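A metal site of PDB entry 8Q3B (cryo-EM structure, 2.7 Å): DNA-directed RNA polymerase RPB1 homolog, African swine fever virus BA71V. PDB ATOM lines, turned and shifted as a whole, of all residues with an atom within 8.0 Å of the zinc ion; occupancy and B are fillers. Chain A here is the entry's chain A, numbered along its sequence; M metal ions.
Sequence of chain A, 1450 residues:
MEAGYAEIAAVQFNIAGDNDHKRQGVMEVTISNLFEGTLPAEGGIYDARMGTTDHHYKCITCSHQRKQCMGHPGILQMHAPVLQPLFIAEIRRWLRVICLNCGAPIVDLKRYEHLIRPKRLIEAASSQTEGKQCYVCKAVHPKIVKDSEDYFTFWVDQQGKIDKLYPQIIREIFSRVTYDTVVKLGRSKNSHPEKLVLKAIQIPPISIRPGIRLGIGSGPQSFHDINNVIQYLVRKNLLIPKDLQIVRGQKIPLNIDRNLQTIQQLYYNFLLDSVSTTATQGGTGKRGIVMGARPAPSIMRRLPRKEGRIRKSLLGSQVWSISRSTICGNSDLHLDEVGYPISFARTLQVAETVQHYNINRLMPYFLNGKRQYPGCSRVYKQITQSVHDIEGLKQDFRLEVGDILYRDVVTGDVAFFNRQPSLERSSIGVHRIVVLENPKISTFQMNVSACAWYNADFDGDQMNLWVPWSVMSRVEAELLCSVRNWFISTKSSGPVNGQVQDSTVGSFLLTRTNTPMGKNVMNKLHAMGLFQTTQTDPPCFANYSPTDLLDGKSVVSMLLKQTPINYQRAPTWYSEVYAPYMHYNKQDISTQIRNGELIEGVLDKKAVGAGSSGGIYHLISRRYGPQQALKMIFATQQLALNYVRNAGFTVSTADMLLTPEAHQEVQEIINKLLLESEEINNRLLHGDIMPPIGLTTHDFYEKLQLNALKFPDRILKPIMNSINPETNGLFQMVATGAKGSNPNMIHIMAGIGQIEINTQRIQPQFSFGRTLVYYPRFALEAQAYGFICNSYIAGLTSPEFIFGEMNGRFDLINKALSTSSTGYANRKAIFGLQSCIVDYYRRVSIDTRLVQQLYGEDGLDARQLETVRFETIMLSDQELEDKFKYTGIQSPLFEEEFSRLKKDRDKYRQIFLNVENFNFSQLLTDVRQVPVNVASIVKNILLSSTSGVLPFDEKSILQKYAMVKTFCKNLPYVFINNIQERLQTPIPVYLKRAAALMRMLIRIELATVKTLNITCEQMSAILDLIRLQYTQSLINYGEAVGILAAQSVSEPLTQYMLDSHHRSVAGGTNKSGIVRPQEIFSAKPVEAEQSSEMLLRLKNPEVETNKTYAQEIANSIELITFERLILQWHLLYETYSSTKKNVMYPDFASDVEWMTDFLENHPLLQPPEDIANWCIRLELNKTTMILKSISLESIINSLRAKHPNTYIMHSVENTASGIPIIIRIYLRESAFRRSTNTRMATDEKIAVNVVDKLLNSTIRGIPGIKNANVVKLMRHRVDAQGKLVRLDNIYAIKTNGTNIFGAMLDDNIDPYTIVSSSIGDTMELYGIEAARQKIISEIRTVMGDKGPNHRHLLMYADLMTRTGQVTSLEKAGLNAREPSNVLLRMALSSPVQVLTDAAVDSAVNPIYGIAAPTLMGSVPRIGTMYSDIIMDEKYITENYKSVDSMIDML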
ATOM      1  N   ILE A  98      -6.798  -4.729  -2.008  1.00  0.00           N
ATOM      2  CA  ILE A  98      -6.075  -5.557  -1.048  1.00  0.00           C
ATOM      3  C   ILE A  98      -6.873  -5.683   0.243  1.00  0.00           C
ATOM      4  O   ILE A  98      -7.642  -4.793   0.618  1.00  0.00           O
ATOM      5  CB  ILE A  98      -4.666  -4.986  -0.780  1.00  0.00           C
ATOM      6  CG1 ILE A  98      -4.748  -3.641  -0.039  1.00  0.00           C
ATOM      7  CG2 ILE A  98      -3.896  -4.846  -2.081  1.00  0.00           C
ATOM      8  CD1 ILE A  98      -3.695  -3.452   1.011  1.00  0.00           C
ATOM      9  N   CYS A  99      -6.697  -6.814   0.924  1.00  0.00           N
ATOM     10  CA  CYS A  99      -7.347  -7.042   2.199  1.00  0.00           C
ATOM     11  C   CYS A  99      -6.806  -6.076   3.253  1.00  0.00           C
ATOM     12  O   CYS A  99      -5.614  -5.785   3.294  1.00  0.00           O
ATOM     13  CB  CYS A  99      -7.135  -8.483   2.650  1.00  0.00           C
ATOM     14  SG  CYS A  99      -7.735  -8.838   4.314  1.00  0.00           S
ATOM     15  N   LEU A 100      -7.704  -5.570   4.095  1.00  0.00           N
ATOM     16  CA  LEU A 100      -7.313  -4.614   5.125  1.00  0.00           C
ATOM     17  C   LEU A 100      -6.750  -5.288   6.374  1.00  0.00           C
ATOM     18  O   LEU A 100      -6.105  -4.599   7.185  1.00  0.00           O
ATOM     19  CB  LEU A 100      -8.507  -3.736   5.515  1.00  0.00           C
ATOM     20  CG  LEU A 100      -8.711  -2.482   4.674  1.00  0.00           C
ATOM     21  CD1 LEU A 100      -8.649  -2.794   3.189  1.00  0.00           C
ATOM     22  CD2 LEU A 100     -10.033  -1.817   5.024  1.00  0.00           C
ATOM     23  N   ASN A 101      -6.966  -6.583   6.549  1.00  0.00           N
ATOM     24  CA  ASN A 101      -6.450  -7.295   7.722  1.00  0.00           C
ATOM     25  C   ASN A 101      -5.114  -7.973   7.437  1.00  0.00           C
ATOM     26  O   ASN A 101      -4.286  -8.096   8.346  1.00  0.00           O
ATOM     27  CB  ASN A 101      -7.461  -8.330   8.202  1.00  0.00           C
ATOM     28  CG  ASN A 101      -6.824  -9.442   8.998  1.00  0.00           C
ATOM     29  OD1 ASN A 101      -6.367  -9.231  10.125  1.00  0.00           O
ATOM     30  ND2 ASN A 101      -6.792 -10.642   8.433  1.00  0.00           N
ATOM     31  N   CYS A 102      -4.896  -8.427   6.201  1.00  0.00           N
ATOM     32  CA  CYS A 102      -3.619  -9.002   5.801  1.00  0.00           C
ATOM     33  C   CYS A 102      -3.162  -8.366   4.500  1.00  0.00           C
ATOM     34  O   CYS A 102      -3.769  -7.388   4.025  1.00  0.00           O
ATOM     35  CB  CYS A 102      -3.733 -10.511   5.662  1.00  0.00           C
ATOM     36  SG  CYS A 102      -4.637 -11.056   4.195  1.00  0.00           S
ATOM     37  N   GLY A 103      -2.102  -8.899   3.902  1.00  0.00           N
ATOM     38  CA  GLY A 103      -1.570  -8.326   2.682  1.00  0.00           C
ATOM     39  C   GLY A 103      -2.085  -8.972   1.411  1.00  0.00           C
ATOM     40  O   GLY A 103      -1.891  -8.437   0.314  1.00  0.00           O
ATOM     41  N   ALA A 104      -2.743 -10.113   1.543  1.00  0.00           N
ATOM     42  CA  ALA A 104      -3.186 -10.839   0.368  1.00  0.00           C
ATOM     43  C   ALA A 104      -4.267 -10.044  -0.371  1.00  0.00           C
ATOM     44  O   ALA A 104      -5.098  -9.395   0.268  1.00  0.00           O
ATOM     45  CB  ALA A 104      -3.730 -12.216   0.763  1.00  0.00           C
ATOM     46  N   PRO A 105      -4.277 -10.075  -1.705  1.00  0.00           N
ATOM     47  CA  PRO A 105      -5.344  -9.398  -2.432  1.00  0.00           C
ATOM     48  C   PRO A 105      -6.652 -10.166  -2.361  1.00  0.00           C
ATOM     49  O   PRO A 105      -6.678 -11.399  -2.302  1.00  0.00           O
ATOM     50  CB  PRO A 105      -4.807  -9.351  -3.865  1.00  0.00           C
ATOM     51  CG  PRO A 105      -3.926 -10.529  -3.971  1.00  0.00           C
ATOM     52  CD  PRO A 105      -3.304 -10.713  -2.605  1.00  0.00           C
ATOM     53  N   ILE A 106      -7.750  -9.409  -2.365  1.00  0.00           N
ATOM     54  CA  ILE A 106      -9.077 -10.019  -2.349  1.00  0.00           C
ATOM     55  C   ILE A 106      -9.587 -10.335  -3.753  1.00  0.00           C
ATOM     56  O   ILE A 106     -10.499 -11.170  -3.891  1.00  0.00           O
ATOM     57  CB  ILE A 106     -10.082  -9.100  -1.624  1.00  0.00           C
ATOM     58  CG1 ILE A 106     -10.514  -7.949  -2.531  1.00  0.00           C
ATOM     59  CG2 ILE A 106      -9.472  -8.591  -0.317  1.00  0.00           C
ATOM     60  CD1 ILE A 106     -11.370  -6.913  -1.846  1.00  0.00           C
ATOM     61  N   GLN A 133     -14.827 -11.983   0.846  1.00  0.00           N
ATOM     62  CA  GLN A 133     -14.067 -12.591   1.934  1.00  0.00           C
ATOM     63  C   GLN A 133     -12.678 -12.970   1.454  1.00  0.00           C
ATOM     64  O   GLN A 133     -12.506 -13.553   0.382  1.00  0.00           O
ATOM     65  CB  GLN A 133     -14.791 -13.830   2.468  1.00  0.00           C
ATOM     66  CG  GLN A 133     -14.170 -14.401   3.739  1.00  0.00           C
ATOM     67  CD  GLN A 133     -13.984 -15.908   3.695  1.00  0.00           C
ATOM     68  OE1 GLN A 133     -14.163 -16.539   2.646  1.00  0.00           O
ATOM     69  NE2 GLN A 133     -13.619 -16.495   4.825  1.00  0.00           N
ATOM     70  N   CYS A 134     -11.673 -12.626   2.265  1.00  0.00           N
ATOM     71  CA  CYS A 134     -10.299 -12.961   1.933  1.00  0.00           C
ATOM     72  C   CYS A 134     -10.079 -14.470   2.033  1.00  0.00           C
ATOM     73  O   CYS A 134     -10.614 -15.130   2.930  1.00  0.00           O
ATOM     74  CB  CYS A 134      -9.343 -12.231   2.869  1.00  0.00           C
ATOM     75  SG  CYS A 134      -7.654 -12.087   2.242  1.00  0.00           S
ATOM     76  N   TYR A 135      -9.304 -15.015   1.097  1.00  0.00           N
ATOM     77  CA  TYR A 135      -9.067 -16.450   1.075  1.00  0.00           C
ATOM     78  C   TYR A 135      -8.111 -16.862   2.197  1.00  0.00           C
ATOM     79  O   TYR A 135      -8.354 -17.854   2.900  1.00  0.00           O
ATOM     80  CB  TYR A 135      -8.513 -16.875  -0.281  1.00  0.00           C
ATOM     81  CG  TYR A 135      -8.248 -18.356  -0.421  1.00  0.00           C
ATOM     82  CD1 TYR A 135      -8.956 -19.286   0.335  1.00  0.00           C
ATOM     83  CD2 TYR A 135      -7.307 -18.827  -1.323  1.00  0.00           C
ATOM     84  CE1 TYR A 135      -8.721 -20.639   0.204  1.00  0.00           C
ATOM     85  CE2 TYR A 135      -7.063 -20.185  -1.464  1.00  0.00           C
ATOM     86  CZ  TYR A 135      -7.775 -21.089  -0.695  1.00  0.00           C
ATOM     87  OH  TYR A 135      -7.537 -22.433  -0.829  1.00  0.00           O
ATOM     88  N   VAL A 136      -7.030 -16.110   2.383  1.00  0.00           N
ATOM     89  CA  VAL A 136      -6.005 -16.513   3.352  1.00  0.00           C
ATOM     90  C   VAL A 136      -6.469 -16.256   4.776  1.00  0.00           C
ATOM     91  O   VAL A 136      -6.048 -16.954   5.707  1.00  0.00           O
ATOM     92  CB  VAL A 136      -4.673 -15.807   3.053  1.00  0.00           C
ATOM     93  CG1 VAL A 136      -4.340 -15.895   1.569  1.00  0.00           C
ATOM     94  CG2 VAL A 136      -4.729 -14.354   3.492  1.00  0.00           C
ATOM     95  N   CYS A 137      -7.320 -15.260   4.996  1.00  0.00           N
ATOM     96  CA  CYS A 137      -7.817 -14.924   6.316  1.00  0.00           C
ATOM     97  C   CYS A 137      -9.334 -14.761   6.270  1.00  0.00           C
ATOM     98  O   CYS A 137      -9.898 -14.393   5.230  1.00  0.00           O
ATOM     99  CB  CYS A 137      -7.169 -13.640   6.852  1.00  0.00           C
ATOM    100  SG  CYS A 137      -7.786 -12.122   6.089  1.00  0.00           S
ATOM    101  N   LYS A 138      -9.979 -15.040   7.400  1.00  0.00           N
ATOM    102  CA  LYS A 138     -11.430 -15.030   7.451  1.00  0.00           C
ATOM    103  C   LYS A 138     -12.028 -13.631   7.366  1.00  0.00           C
ATOM    104  O   LYS A 138     -13.245 -13.513   7.217  1.00  0.00           O
ATOM    105  CB  LYS A 138     -11.911 -15.713   8.727  1.00  0.00           C
ATOM    106  CG  LYS A 138     -11.489 -17.177   8.862  1.00  0.00           C
ATOM    107  CD  LYS A 138     -12.105 -18.059   7.786  1.00  0.00           C
ATOM    108  CE  LYS A 138     -13.617 -18.174   7.939  1.00  0.00           C
ATOM    109  NZ  LYS A 138     -14.202 -19.145   6.968  1.00  0.00           N
ATOM    110  N   ALA A 139     -11.205 -12.588   7.457  1.00  0.00           N
ATOM    111  CA  ALA A 139     -11.737 -11.231   7.416  1.00  0.00           C
ATOM    112  C   ALA A 139     -12.438 -10.963   6.092  1.00  0.00           C
ATOM    113  O   ALA A 139     -11.995 -11.423   5.041  1.00  0.00           O
ATOM    114  CB  ALA A 139     -10.609 -10.221   7.633  1.00  0.00           C
ATOM    115  N   VAL A 140     -13.532 -10.217   6.155  1.00  0.00           N
ATOM    116  CA  VAL A 140     -14.305  -9.840   4.980  1.00  0.00           C
ATOM    117  C   VAL A 140     -13.997  -8.395   4.637  1.00  0.00           C
ATOM    118  O   VAL A 140     -13.964  -7.530   5.525  1.00  0.00           O
ATOM    119  CB  VAL A 140     -15.821 -10.046   5.213  1.00  0.00           C
ATOM    120  CG1 VAL A 140     -16.409  -8.889   6.006  1.00  0.00           C
ATOM    121  CG2 VAL A 140     -16.534 -10.207   3.884  1.00  0.00           C
ATOM    122  N   HIS A 141     -13.761  -8.124   3.359  1.00  0.00           N
ATOM    123  CA  HIS A 141     -13.355  -6.791   2.938  1.00  0.00           C
ATOM    124  C   HIS A 141     -14.499  -5.802   3.147  1.00  0.00           C
ATOM    125  O   HIS A 141     -15.598  -6.012   2.610  1.00  0.00           O
ATOM    126  CB  HIS A 141     -12.939  -6.806   1.470  1.00  0.00           C
ATOM    127  CG  HIS A 141     -12.205  -5.572   1.053  1.00  0.00           C
ATOM    128  ND1 HIS A 141     -12.698  -4.694   0.101  1.00  0.00           N
ATOM    129  CD2 HIS A 141     -11.007  -5.067   1.442  1.00  0.00           C
ATOM    130  CE1 HIS A 141     -11.841  -3.702  -0.064  1.00  0.00           C
ATOM    131  NE2 HIS A 141     -10.806  -3.906   0.737  1.00  0.00           N
HETATM  132 ZN    ZN M   1      -6.967 -11.027   4.205  1.00  0.00          ZN
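Four residues have an atom within 4 Å of the zinc ion: Cys 99, Cys 102, Cys 134 and Cys 137.
The zinc ion is bound by the side-chain sulfur (SG) of Cys 99 (2.3 Å), the side-chain sulfur (SG) of Cys 137 (2.3 Å), the side-chain sulfur (SG) of Cys 102 (2.3 Å) and the side-chain sulfur (SG) of Cys 134 (2.3 Å).
The zinc ion has four donor atoms within binding distance.
SG of Cys 137 lies close to ND2 of Asn 101, 2.9 Å away.
The backbone NH of Cys 134 lies within hydrogen-bond range of the backbone carbonyl oxygen of Ala 139 (3.0 Å).
SG of Cys 137 lies close to N of Ala 139, at 3.7 Å.
The side-chain sulfur (SG) of Cys 99 lies close to the backbone NH (N) of Asn 101.
N of Ala 104 sits close to SG of Cys 102 (3.4 Å).
The backbone NH of Cys 99 is in hydrogen-bond range of the backbone carbonyl oxygen of Ala 104.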
